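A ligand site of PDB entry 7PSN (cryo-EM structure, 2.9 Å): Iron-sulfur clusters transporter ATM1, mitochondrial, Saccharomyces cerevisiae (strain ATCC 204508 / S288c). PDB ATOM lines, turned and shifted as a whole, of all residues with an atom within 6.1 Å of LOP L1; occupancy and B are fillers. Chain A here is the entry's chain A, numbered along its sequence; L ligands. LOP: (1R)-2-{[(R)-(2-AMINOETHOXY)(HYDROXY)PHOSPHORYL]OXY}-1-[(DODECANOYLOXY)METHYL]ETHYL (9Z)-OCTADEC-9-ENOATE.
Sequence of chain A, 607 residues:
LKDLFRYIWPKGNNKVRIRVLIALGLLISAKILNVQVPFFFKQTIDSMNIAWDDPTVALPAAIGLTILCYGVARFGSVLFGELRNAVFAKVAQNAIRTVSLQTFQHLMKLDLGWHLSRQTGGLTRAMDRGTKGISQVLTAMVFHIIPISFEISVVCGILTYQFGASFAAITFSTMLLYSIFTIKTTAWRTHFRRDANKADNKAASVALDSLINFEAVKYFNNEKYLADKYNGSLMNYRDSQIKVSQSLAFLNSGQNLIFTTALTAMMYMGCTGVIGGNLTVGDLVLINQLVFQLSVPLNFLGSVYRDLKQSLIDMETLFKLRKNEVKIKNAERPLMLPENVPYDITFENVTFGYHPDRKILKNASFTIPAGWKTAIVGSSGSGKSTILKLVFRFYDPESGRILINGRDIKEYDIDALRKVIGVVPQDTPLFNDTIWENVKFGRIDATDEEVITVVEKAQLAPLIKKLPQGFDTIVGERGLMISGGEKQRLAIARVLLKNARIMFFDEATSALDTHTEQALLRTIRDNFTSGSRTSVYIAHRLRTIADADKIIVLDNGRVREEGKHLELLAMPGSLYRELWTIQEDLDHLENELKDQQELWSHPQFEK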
ATOM      1  N   ILE A  28     -24.121  16.250  14.926  1.00  0.00           N
ATOM      2  CA  ILE A  28     -23.269  16.921  15.896  1.00  0.00           C
ATOM      3  C   ILE A  28     -21.886  17.147  15.306  1.00  0.00           C
ATOM      4  O   ILE A  28     -21.374  18.273  15.309  1.00  0.00           O
ATOM      5  CB  ILE A  28     -23.187  16.085  17.189  1.00  0.00           C
ATOM      6  CG1 ILE A  28     -24.544  16.019  17.884  1.00  0.00           C
ATOM      7  CG2 ILE A  28     -22.148  16.662  18.116  1.00  0.00           C
ATOM      8  CD1 ILE A  28     -25.068  17.325  18.379  1.00  0.00           C
ATOM      9  N   ILE A  32     -19.784  20.547  14.409  1.00  0.00           N
ATOM     10  CA  ILE A  32     -18.515  20.793  15.081  1.00  0.00           C
ATOM     11  C   ILE A  32     -17.456  21.188  14.072  1.00  0.00           C
ATOM     12  O   ILE A  32     -16.703  22.157  14.263  1.00  0.00           O
ATOM     13  CB  ILE A  32     -18.080  19.565  15.902  1.00  0.00           C
ATOM     14  CG1 ILE A  32     -18.983  19.365  17.119  1.00  0.00           C
ATOM     15  CG2 ILE A  32     -16.651  19.714  16.340  1.00  0.00           C
ATOM     16  CD1 ILE A  32     -19.263  20.606  17.915  1.00  0.00           C
ATOM     17  N   VAL A  35     -18.025  24.557  12.552  1.00  0.00           N
ATOM     18  CA  VAL A  35     -17.654  25.619  13.475  1.00  0.00           C
ATOM     19  C   VAL A  35     -16.154  25.693  13.704  1.00  0.00           C
ATOM     20  O   VAL A  35     -15.660  26.741  14.147  1.00  0.00           O
ATOM     21  CB  VAL A  35     -18.370  25.415  14.824  1.00  0.00           C
ATOM     22  CG1 VAL A  35     -17.829  26.364  15.851  1.00  0.00           C
ATOM     23  CG2 VAL A  35     -19.851  25.600  14.668  1.00  0.00           C
ATOM     24  N   GLN A  36     -15.420  24.632  13.423  1.00  0.00           N
ATOM     25  CA  GLN A  36     -13.983  24.616  13.629  1.00  0.00           C
ATOM     26  C   GLN A  36     -13.202  25.113  12.419  1.00  0.00           C
ATOM     27  O   GLN A  36     -12.084  25.596  12.582  1.00  0.00           O
ATOM     28  CB  GLN A  36     -13.522  23.198  13.983  1.00  0.00           C
ATOM     29  CG  GLN A  36     -12.064  23.057  14.313  1.00  0.00           C
ATOM     30  CD  GLN A  36     -11.684  23.741  15.597  1.00  0.00           C
ATOM     31  OE1 GLN A  36     -10.931  24.710  15.613  1.00  0.00           O
ATOM     32  NE2 GLN A  36     -12.244  23.258  16.691  1.00  0.00           N
ATOM     33  N   PHE A  39     -11.590  28.584  12.568  1.00  0.00           N
ATOM     34  CA  PHE A  39     -10.388  28.728  13.390  1.00  0.00           C
ATOM     35  C   PHE A  39      -9.139  28.387  12.586  1.00  0.00           C
ATOM     36  O   PHE A  39      -8.107  29.051  12.720  1.00  0.00           O
ATOM     37  CB  PHE A  39     -10.493  27.838  14.617  1.00  0.00           C
ATOM     38  CG  PHE A  39     -11.465  28.335  15.639  1.00  0.00           C
ATOM     39  CD1 PHE A  39     -12.803  28.008  15.560  1.00  0.00           C
ATOM     40  CD2 PHE A  39     -11.044  29.131  16.677  1.00  0.00           C
ATOM     41  CE1 PHE A  39     -13.698  28.466  16.502  1.00  0.00           C
ATOM     42  CE2 PHE A  39     -11.935  29.602  17.620  1.00  0.00           C
ATOM     43  CZ  PHE A  39     -13.260  29.260  17.522  1.00  0.00           C
ATOM     44  N   LYS A  42      -8.525  31.415  10.475  1.00  0.00           N
ATOM     45  CA  LYS A  42      -7.870  32.446  11.259  1.00  0.00           C
ATOM     46  C   LYS A  42      -6.390  32.124  11.471  1.00  0.00           C
ATOM     47  O   LYS A  42      -5.542  33.030  11.429  1.00  0.00           O
ATOM     48  CB  LYS A  42      -8.569  32.589  12.608  1.00  0.00           C
ATOM     49  CG  LYS A  42      -7.791  33.402  13.619  1.00  0.00           C
ATOM     50  CD  LYS A  42      -8.508  33.456  14.944  1.00  0.00           C
ATOM     51  CE  LYS A  42      -7.805  32.640  15.999  1.00  0.00           C
ATOM     52  NZ  LYS A  42      -8.181  33.064  17.364  1.00  0.00           N
ATOM     53  N   GLN A  43      -6.066  30.861  11.731  1.00  0.00           N
ATOM     54  CA  GLN A  43      -4.677  30.493  11.940  1.00  0.00           C
ATOM     55  C   GLN A  43      -3.847  30.779  10.696  1.00  0.00           C
ATOM     56  O   GLN A  43      -2.772  31.386  10.781  1.00  0.00           O
ATOM     57  CB  GLN A  43      -4.573  29.012  12.324  1.00  0.00           C
ATOM     58  CG  GLN A  43      -5.001  28.710  13.743  1.00  0.00           C
ATOM     59  CD  GLN A  43      -4.779  27.270  14.126  1.00  0.00           C
ATOM     60  OE1 GLN A  43      -3.938  26.581  13.538  1.00  0.00           O
ATOM     61  NE2 GLN A  43      -5.526  26.801  15.111  1.00  0.00           N
ATOM     62  N   ILE A 146     -32.684  21.761  13.541  1.00  0.00           N
ATOM     63  CA  ILE A 146     -31.922  21.290  14.696  1.00  0.00           C
ATOM     64  C   ILE A 146     -30.455  21.628  14.485  1.00  0.00           C
ATOM     65  O   ILE A 146     -29.781  22.105  15.418  1.00  0.00           O
ATOM     66  CB  ILE A 146     -32.117  19.790  14.934  1.00  0.00           C
ATOM     67  CG1 ILE A 146     -33.556  19.512  15.353  1.00  0.00           C
ATOM     68  CG2 ILE A 146     -31.168  19.293  16.003  1.00  0.00           C
ATOM     69  CD1 ILE A 146     -33.894  18.061  15.423  1.00  0.00           C
ATOM     70  N   SER A 149     -29.842  25.232  15.036  1.00  0.00           N
ATOM     71  CA  SER A 149     -29.991  25.550  16.457  1.00  0.00           C
ATOM     72  C   SER A 149     -28.744  25.186  17.233  1.00  0.00           C
ATOM     73  O   SER A 149     -28.260  25.970  18.057  1.00  0.00           O
ATOM     74  CB  SER A 149     -31.211  24.822  17.027  1.00  0.00           C
ATOM     75  OG  SER A 149     -32.316  24.899  16.147  1.00  0.00           O
ATOM     76  N   PHE A 150     -28.207  23.989  16.999  1.00  0.00           N
ATOM     77  CA  PHE A 150     -26.975  23.583  17.654  1.00  0.00           C
ATOM     78  C   PHE A 150     -25.831  24.531  17.288  1.00  0.00           C
ATOM     79  O   PHE A 150     -25.019  24.899  18.134  1.00  0.00           O
ATOM     80  CB  PHE A 150     -26.642  22.144  17.270  1.00  0.00           C
ATOM     81  CG  PHE A 150     -25.432  21.592  17.945  1.00  0.00           C
ATOM     82  CD1 PHE A 150     -25.471  21.233  19.275  1.00  0.00           C
ATOM     83  CD2 PHE A 150     -24.252  21.418  17.248  1.00  0.00           C
ATOM     84  CE1 PHE A 150     -24.347  20.715  19.905  1.00  0.00           C
ATOM     85  CE2 PHE A 150     -23.139  20.905  17.867  1.00  0.00           C
ATOM     86  CZ  PHE A 150     -23.183  20.556  19.196  1.00  0.00           C
ATOM     87  N   SER A 153     -26.207  27.776  19.124  1.00  0.00           N
ATOM     88  CA  SER A 153     -25.831  27.612  20.520  1.00  0.00           C
ATOM     89  C   SER A 153     -24.326  27.643  20.684  1.00  0.00           C
ATOM     90  O   SER A 153     -23.787  28.376  21.534  1.00  0.00           O
ATOM     91  CB  SER A 153     -26.399  26.300  21.050  1.00  0.00           C
ATOM     92  OG  SER A 153     -27.788  26.206  20.790  1.00  0.00           O
ATOM     93  N   VAL A 154     -23.607  26.856  19.875  1.00  0.00           N
ATOM     94  CA  VAL A 154     -22.160  26.799  20.038  1.00  0.00           C
ATOM     95  C   VAL A 154     -21.510  28.120  19.619  1.00  0.00           C
ATOM     96  O   VAL A 154     -20.483  28.511  20.174  1.00  0.00           O
ATOM     97  CB  VAL A 154     -21.558  25.624  19.255  1.00  0.00           C
ATOM     98  CG1 VAL A 154     -22.209  24.326  19.677  1.00  0.00           C
ATOM     99  CG2 VAL A 154     -21.726  25.829  17.783  1.00  0.00           C
ATOM    100  N   GLY A 157     -21.882  30.398  22.512  1.00  0.00           N
ATOM    101  CA  GLY A 157     -20.912  30.003  23.524  1.00  0.00           C
ATOM    102  C   GLY A 157     -19.502  30.469  23.191  1.00  0.00           C
ATOM    103  O   GLY A 157     -18.782  30.958  24.053  1.00  0.00           O
ATOM    104  N   ILE A 158     -19.094  30.309  21.924  1.00  0.00           N
ATOM    105  CA  ILE A 158     -17.747  30.685  21.527  1.00  0.00           C
ATOM    106  C   ILE A 158     -17.557  32.184  21.658  1.00  0.00           C
ATOM    107  O   ILE A 158     -16.564  32.658  22.225  1.00  0.00           O
ATOM    108  CB  ILE A 158     -17.458  30.215  20.098  1.00  0.00           C
ATOM    109  CG1 ILE A 158     -17.401  28.700  20.027  1.00  0.00           C
ATOM    110  CG2 ILE A 158     -16.158  30.793  19.610  1.00  0.00           C
ATOM    111  CD1 ILE A 158     -17.517  28.164  18.640  1.00  0.00           C
ATOM    112  N   TYR A 161     -17.249  33.114  25.255  1.00  0.00           N
ATOM    113  CA  TYR A 161     -16.098  32.598  25.994  1.00  0.00           C
ATOM    114  C   TYR A 161     -14.773  33.133  25.497  1.00  0.00           C
ATOM    115  O   TYR A 161     -13.806  33.175  26.268  1.00  0.00           O
ATOM    116  CB  TYR A 161     -16.090  31.068  25.921  1.00  0.00           C
ATOM    117  CG  TYR A 161     -14.755  30.434  26.245  1.00  0.00           C
ATOM    118  CD1 TYR A 161     -14.405  30.144  27.550  1.00  0.00           C
ATOM    119  CD2 TYR A 161     -13.852  30.127  25.239  1.00  0.00           C
ATOM    120  CE1 TYR A 161     -13.184  29.564  27.845  1.00  0.00           C
ATOM    121  CE2 TYR A 161     -12.637  29.544  25.522  1.00  0.00           C
ATOM    122  CZ  TYR A 161     -12.314  29.262  26.822  1.00  0.00           C
ATOM    123  OH  TYR A 161     -11.101  28.677  27.115  1.00  0.00           O
ATOM    124  N   GLN A 162     -14.689  33.548  24.234  1.00  0.00           N
ATOM    125  CA  GLN A 162     -13.415  33.909  23.615  1.00  0.00           C
ATOM    126  C   GLN A 162     -13.250  35.405  23.370  1.00  0.00           C
ATOM    127  O   GLN A 162     -12.115  35.851  23.194  1.00  0.00           O
ATOM    128  CB  GLN A 162     -13.254  33.169  22.284  1.00  0.00           C
ATOM    129  CG  GLN A 162     -11.865  32.631  22.043  1.00  0.00           C
ATOM    130  CD  GLN A 162     -11.767  31.824  20.774  1.00  0.00           C
ATOM    131  OE1 GLN A 162     -12.715  31.746  20.002  1.00  0.00           O
ATOM    132  NE2 GLN A 162     -10.603  31.225  20.541  1.00  0.00           N
HETATM  133  N1  LOP L   1      -9.095  26.339  24.516  1.00  0.00           N
HETATM  134  C1  LOP L   1      -9.240  27.707  24.029  1.00  0.00           C
HETATM  135  C2  LOP L   1      -8.513  27.928  22.735  1.00  0.00           C
HETATM  136  O1  LOP L   1      -9.444  27.769  21.620  1.00  0.00           O
HETATM  137  P1  LOP L   1      -8.861  27.611  20.132  1.00  0.00           P
HETATM  138  O2  LOP L   1     -10.030  26.819  19.370  1.00  0.00           O
HETATM  139  O3  LOP L   1      -7.677  26.683  20.206  1.00  0.00           O
HETATM  140  O4  LOP L   1      -8.686  28.977  19.536  1.00  0.00           O
HETATM  141  C3  LOP L   1     -10.918  25.960  20.128  1.00  0.00           C
HETATM  142  C4  LOP L   1     -12.343  26.434  19.933  1.00  0.00           C
HETATM  143  C5  LOP L   1     -13.064  25.718  18.821  1.00  0.00           C
HETATM  144  O5  LOP L   1     -13.096  26.335  21.173  1.00  0.00           O
HETATM  145  O6  LOP L   1     -13.737  24.555  19.366  1.00  0.00           O
HETATM  146  C6  LOP L   1     -13.278  27.458  21.873  1.00  0.00           C
HETATM  147  O7  LOP L   1     -12.405  28.264  22.020  1.00  0.00           O
HETATM  148  C7  LOP L   1     -14.653  27.586  22.432  1.00  0.00           C
HETATM  149  C8  LOP L   1     -15.080  26.405  23.221  1.00  0.00           C
HETATM  150  C9  LOP L   1     -16.436  26.610  23.864  1.00  0.00           C
HETATM  151  C10 LOP L   1     -17.566  26.031  23.062  1.00  0.00           C
HETATM  152  C11 LOP L   1     -18.910  26.310  23.643  1.00  0.00           C
HETATM  153  C12 LOP L   1     -19.943  25.240  23.352  1.00  0.00           C
HETATM  154  C13 LOP L   1     -21.258  25.467  24.016  1.00  0.00           C
HETATM  155  C14 LOP L   1     -22.302  24.493  23.579  1.00  0.00           C
HETATM  156  C15 LOP L   1     -23.553  24.787  23.391  1.00  0.00           C
HETATM  157  C16 LOP L   1     -24.712  23.910  23.762  1.00  0.00           C
HETATM  158  C17 LOP L   1     -25.228  23.099  22.631  1.00  0.00           C
HETATM  159  C18 LOP L   1     -26.425  22.237  22.986  1.00  0.00           C
HETATM  160  C19 LOP L   1     -27.752  22.773  22.520  1.00  0.00           C
HETATM  161  C20 LOP L   1     -28.717  21.704  22.059  1.00  0.00           C
HETATM  162  C21 LOP L   1     -29.959  22.229  21.383  1.00  0.00           C
HETATM  163  C22 LOP L   1     -30.563  21.281  20.373  1.00  0.00           C
HETATM  164  C23 LOP L   1     -31.953  21.660  19.929  1.00  0.00           C
HETATM  165  C24 LOP L   1     -14.840  24.181  18.756  1.00  0.00           C
HETATM  166  O8  LOP L   1     -14.869  23.737  17.643  1.00  0.00           O
HETATM  167  C25 LOP L   1     -16.045  24.364  19.613  1.00  0.00           C
HETATM  168  C26 LOP L   1     -17.202  23.579  19.142  1.00  0.00           C
HETATM  169  C27 LOP L   1     -18.131  23.207  20.273  1.00  0.00           C
HETATM  170  C28 LOP L   1     -17.510  22.268  21.267  1.00  0.00           C
HETATM  171  C29 LOP L   1     -18.473  21.257  21.860  1.00  0.00           C
HETATM  172  C30 LOP L   1     -19.908  21.489  21.482  1.00  0.00           C
HETATM  173  C31 LOP L   1     -20.895  20.839  22.418  1.00  0.00           C
HETATM  174  C32 LOP L   1     -21.226  19.413  22.060  1.00  0.00           C
HETATM  175  C33 LOP L   1     -22.488  18.900  22.716  1.00  0.00           C
HETATM  176  C34 LOP L   1     -22.997  17.596  22.180  1.00  0.00           C
HETATM  177  C35 LOP L   1     -24.495  17.423  22.352  1.00  0.00           C
HETATM  178  N1  LOP L   2     -11.545  33.794  29.192  1.00  0.00           N
HETATM  179  C1  LOP L   2     -11.672  34.776  28.132  1.00  0.00           C
HETATM  180  C2  LOP L   2     -12.681  35.840  28.530  1.00  0.00           C
HETATM  181  O1  LOP L   2     -13.380  35.419  29.673  1.00  0.00           O
HETATM  182  P1  LOP L   2     -14.752  36.225  30.111  1.00  0.00           P
HETATM  183  O2  LOP L   2     -16.079  35.397  29.580  1.00  0.00           O
HETATM  184  O3  LOP L   2     -14.742  37.607  29.493  1.00  0.00           O
HETATM  185  O4  LOP L   2     -14.812  36.353  31.613  1.00  0.00           O
HETATM  186  C3  LOP L   2     -16.116  34.012  29.781  1.00  0.00           C
HETATM  187  C4  LOP L   2     -17.561  33.516  29.651  1.00  0.00           C
HETATM  188  C5  LOP L   2     -17.593  31.999  29.613  1.00  0.00           C
HETATM  189  O5  LOP L   2     -18.308  33.973  30.736  1.00  0.00           O
HETATM  190  O6  LOP L   2     -18.858  31.553  30.019  1.00  0.00           O
HETATM  191  C6  LOP L   2     -19.207  34.992  30.413  1.00  0.00           C
HETATM  192  O7  LOP L   2     -18.793  36.055  30.080  1.00  0.00           O
HETATM  193  C7  LOP L   2     -20.705  34.740  30.483  1.00  0.00           C
HETATM  194  C8  LOP L   2     -21.458  36.005  30.083  1.00  0.00           C
HETATM  195  C9  LOP L   2     -22.942  35.828  30.391  1.00  0.00           C
HETATM  196  C10 LOP L   2     -23.596  34.933  29.335  1.00  0.00           C
HETATM  197  C11 LOP L   2     -24.012  33.587  29.923  1.00  0.00           C
HETATM  198  C12 LOP L   2     -25.268  33.100  29.197  1.00  0.00           C
HETATM  199  C24 LOP L   2     -19.466  30.626  29.154  1.00  0.00           C
HETATM  200  O8  LOP L   2     -18.819  29.812  28.584  1.00  0.00           O
HETATM  201  C25 LOP L   2     -20.984  30.656  28.963  1.00  0.00           C
HETATM  202  C26 LOP L   2     -21.367  29.778  27.771  1.00  0.00           C
HETATM  203  C27 LOP L   2     -22.768  30.141  27.312  1.00  0.00           C
HETATM  204  C28 LOP L   2     -23.674  28.911  27.379  1.00  0.00           C
HETATM  205  C29 LOP L   2     -24.013  28.440  25.963  1.00  0.00           C
HETATM  206  C30 LOP L   2     -25.415  28.892  25.596  1.00  0.00           C
HETATM  207  C31 LOP L   2     -26.344  27.684  25.578  1.00  0.00           C
HETATM  208  C32 LOP L   2     -27.780  28.130  25.306  1.00  0.00           C
HETATM  209  C33 LOP L   2     -27.814  29.071  24.107  1.00  0.00           C
HETATM  210  C34 LOP L   2     -29.255  29.367  23.714  1.00  0.00           C
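Ile 32 touches LOP L1 (CD1 to C27, 3.7 Å).
CE1 of Phe 39 touches C5 of LOP L1, 3.7 Å away.
Phe 150 touches LOP L1.
Ser 153 touches LOP L1.
Val 154 touches LOP L1.
Ile 158 touches LOP L1.
Tyr 161 touches LOP L1 (OH to C1, 3.7 Å).
Hydrophobic or aromatic side chains within 4 Å of LOP L1: Ile 32, Phe 39, Phe 150, Val 154, Ile 158 and Tyr 161.
Along chain A the residues within 4 Å of LOP L1 span positions 32 to 162.
The nearest printed residue that does not touch LOP L1 is Ile 28 (4.02 Å).
The side-chain hydroxyl of Ser 153 sits at hydrogen-bond distance from the backbone carbonyl oxygen of Ser 149 (2.8 Å).
An oxygen (O8) of LOP L1 sits at hydrogen-bond distance from the side-chain amide nitrogen of Gln 36 (2.8 Å).
An oxygen (O4) of LOP L1 sits at hydrogen-bond distance from the side-chain amide nitrogen of Gln 162 (3.1 Å).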
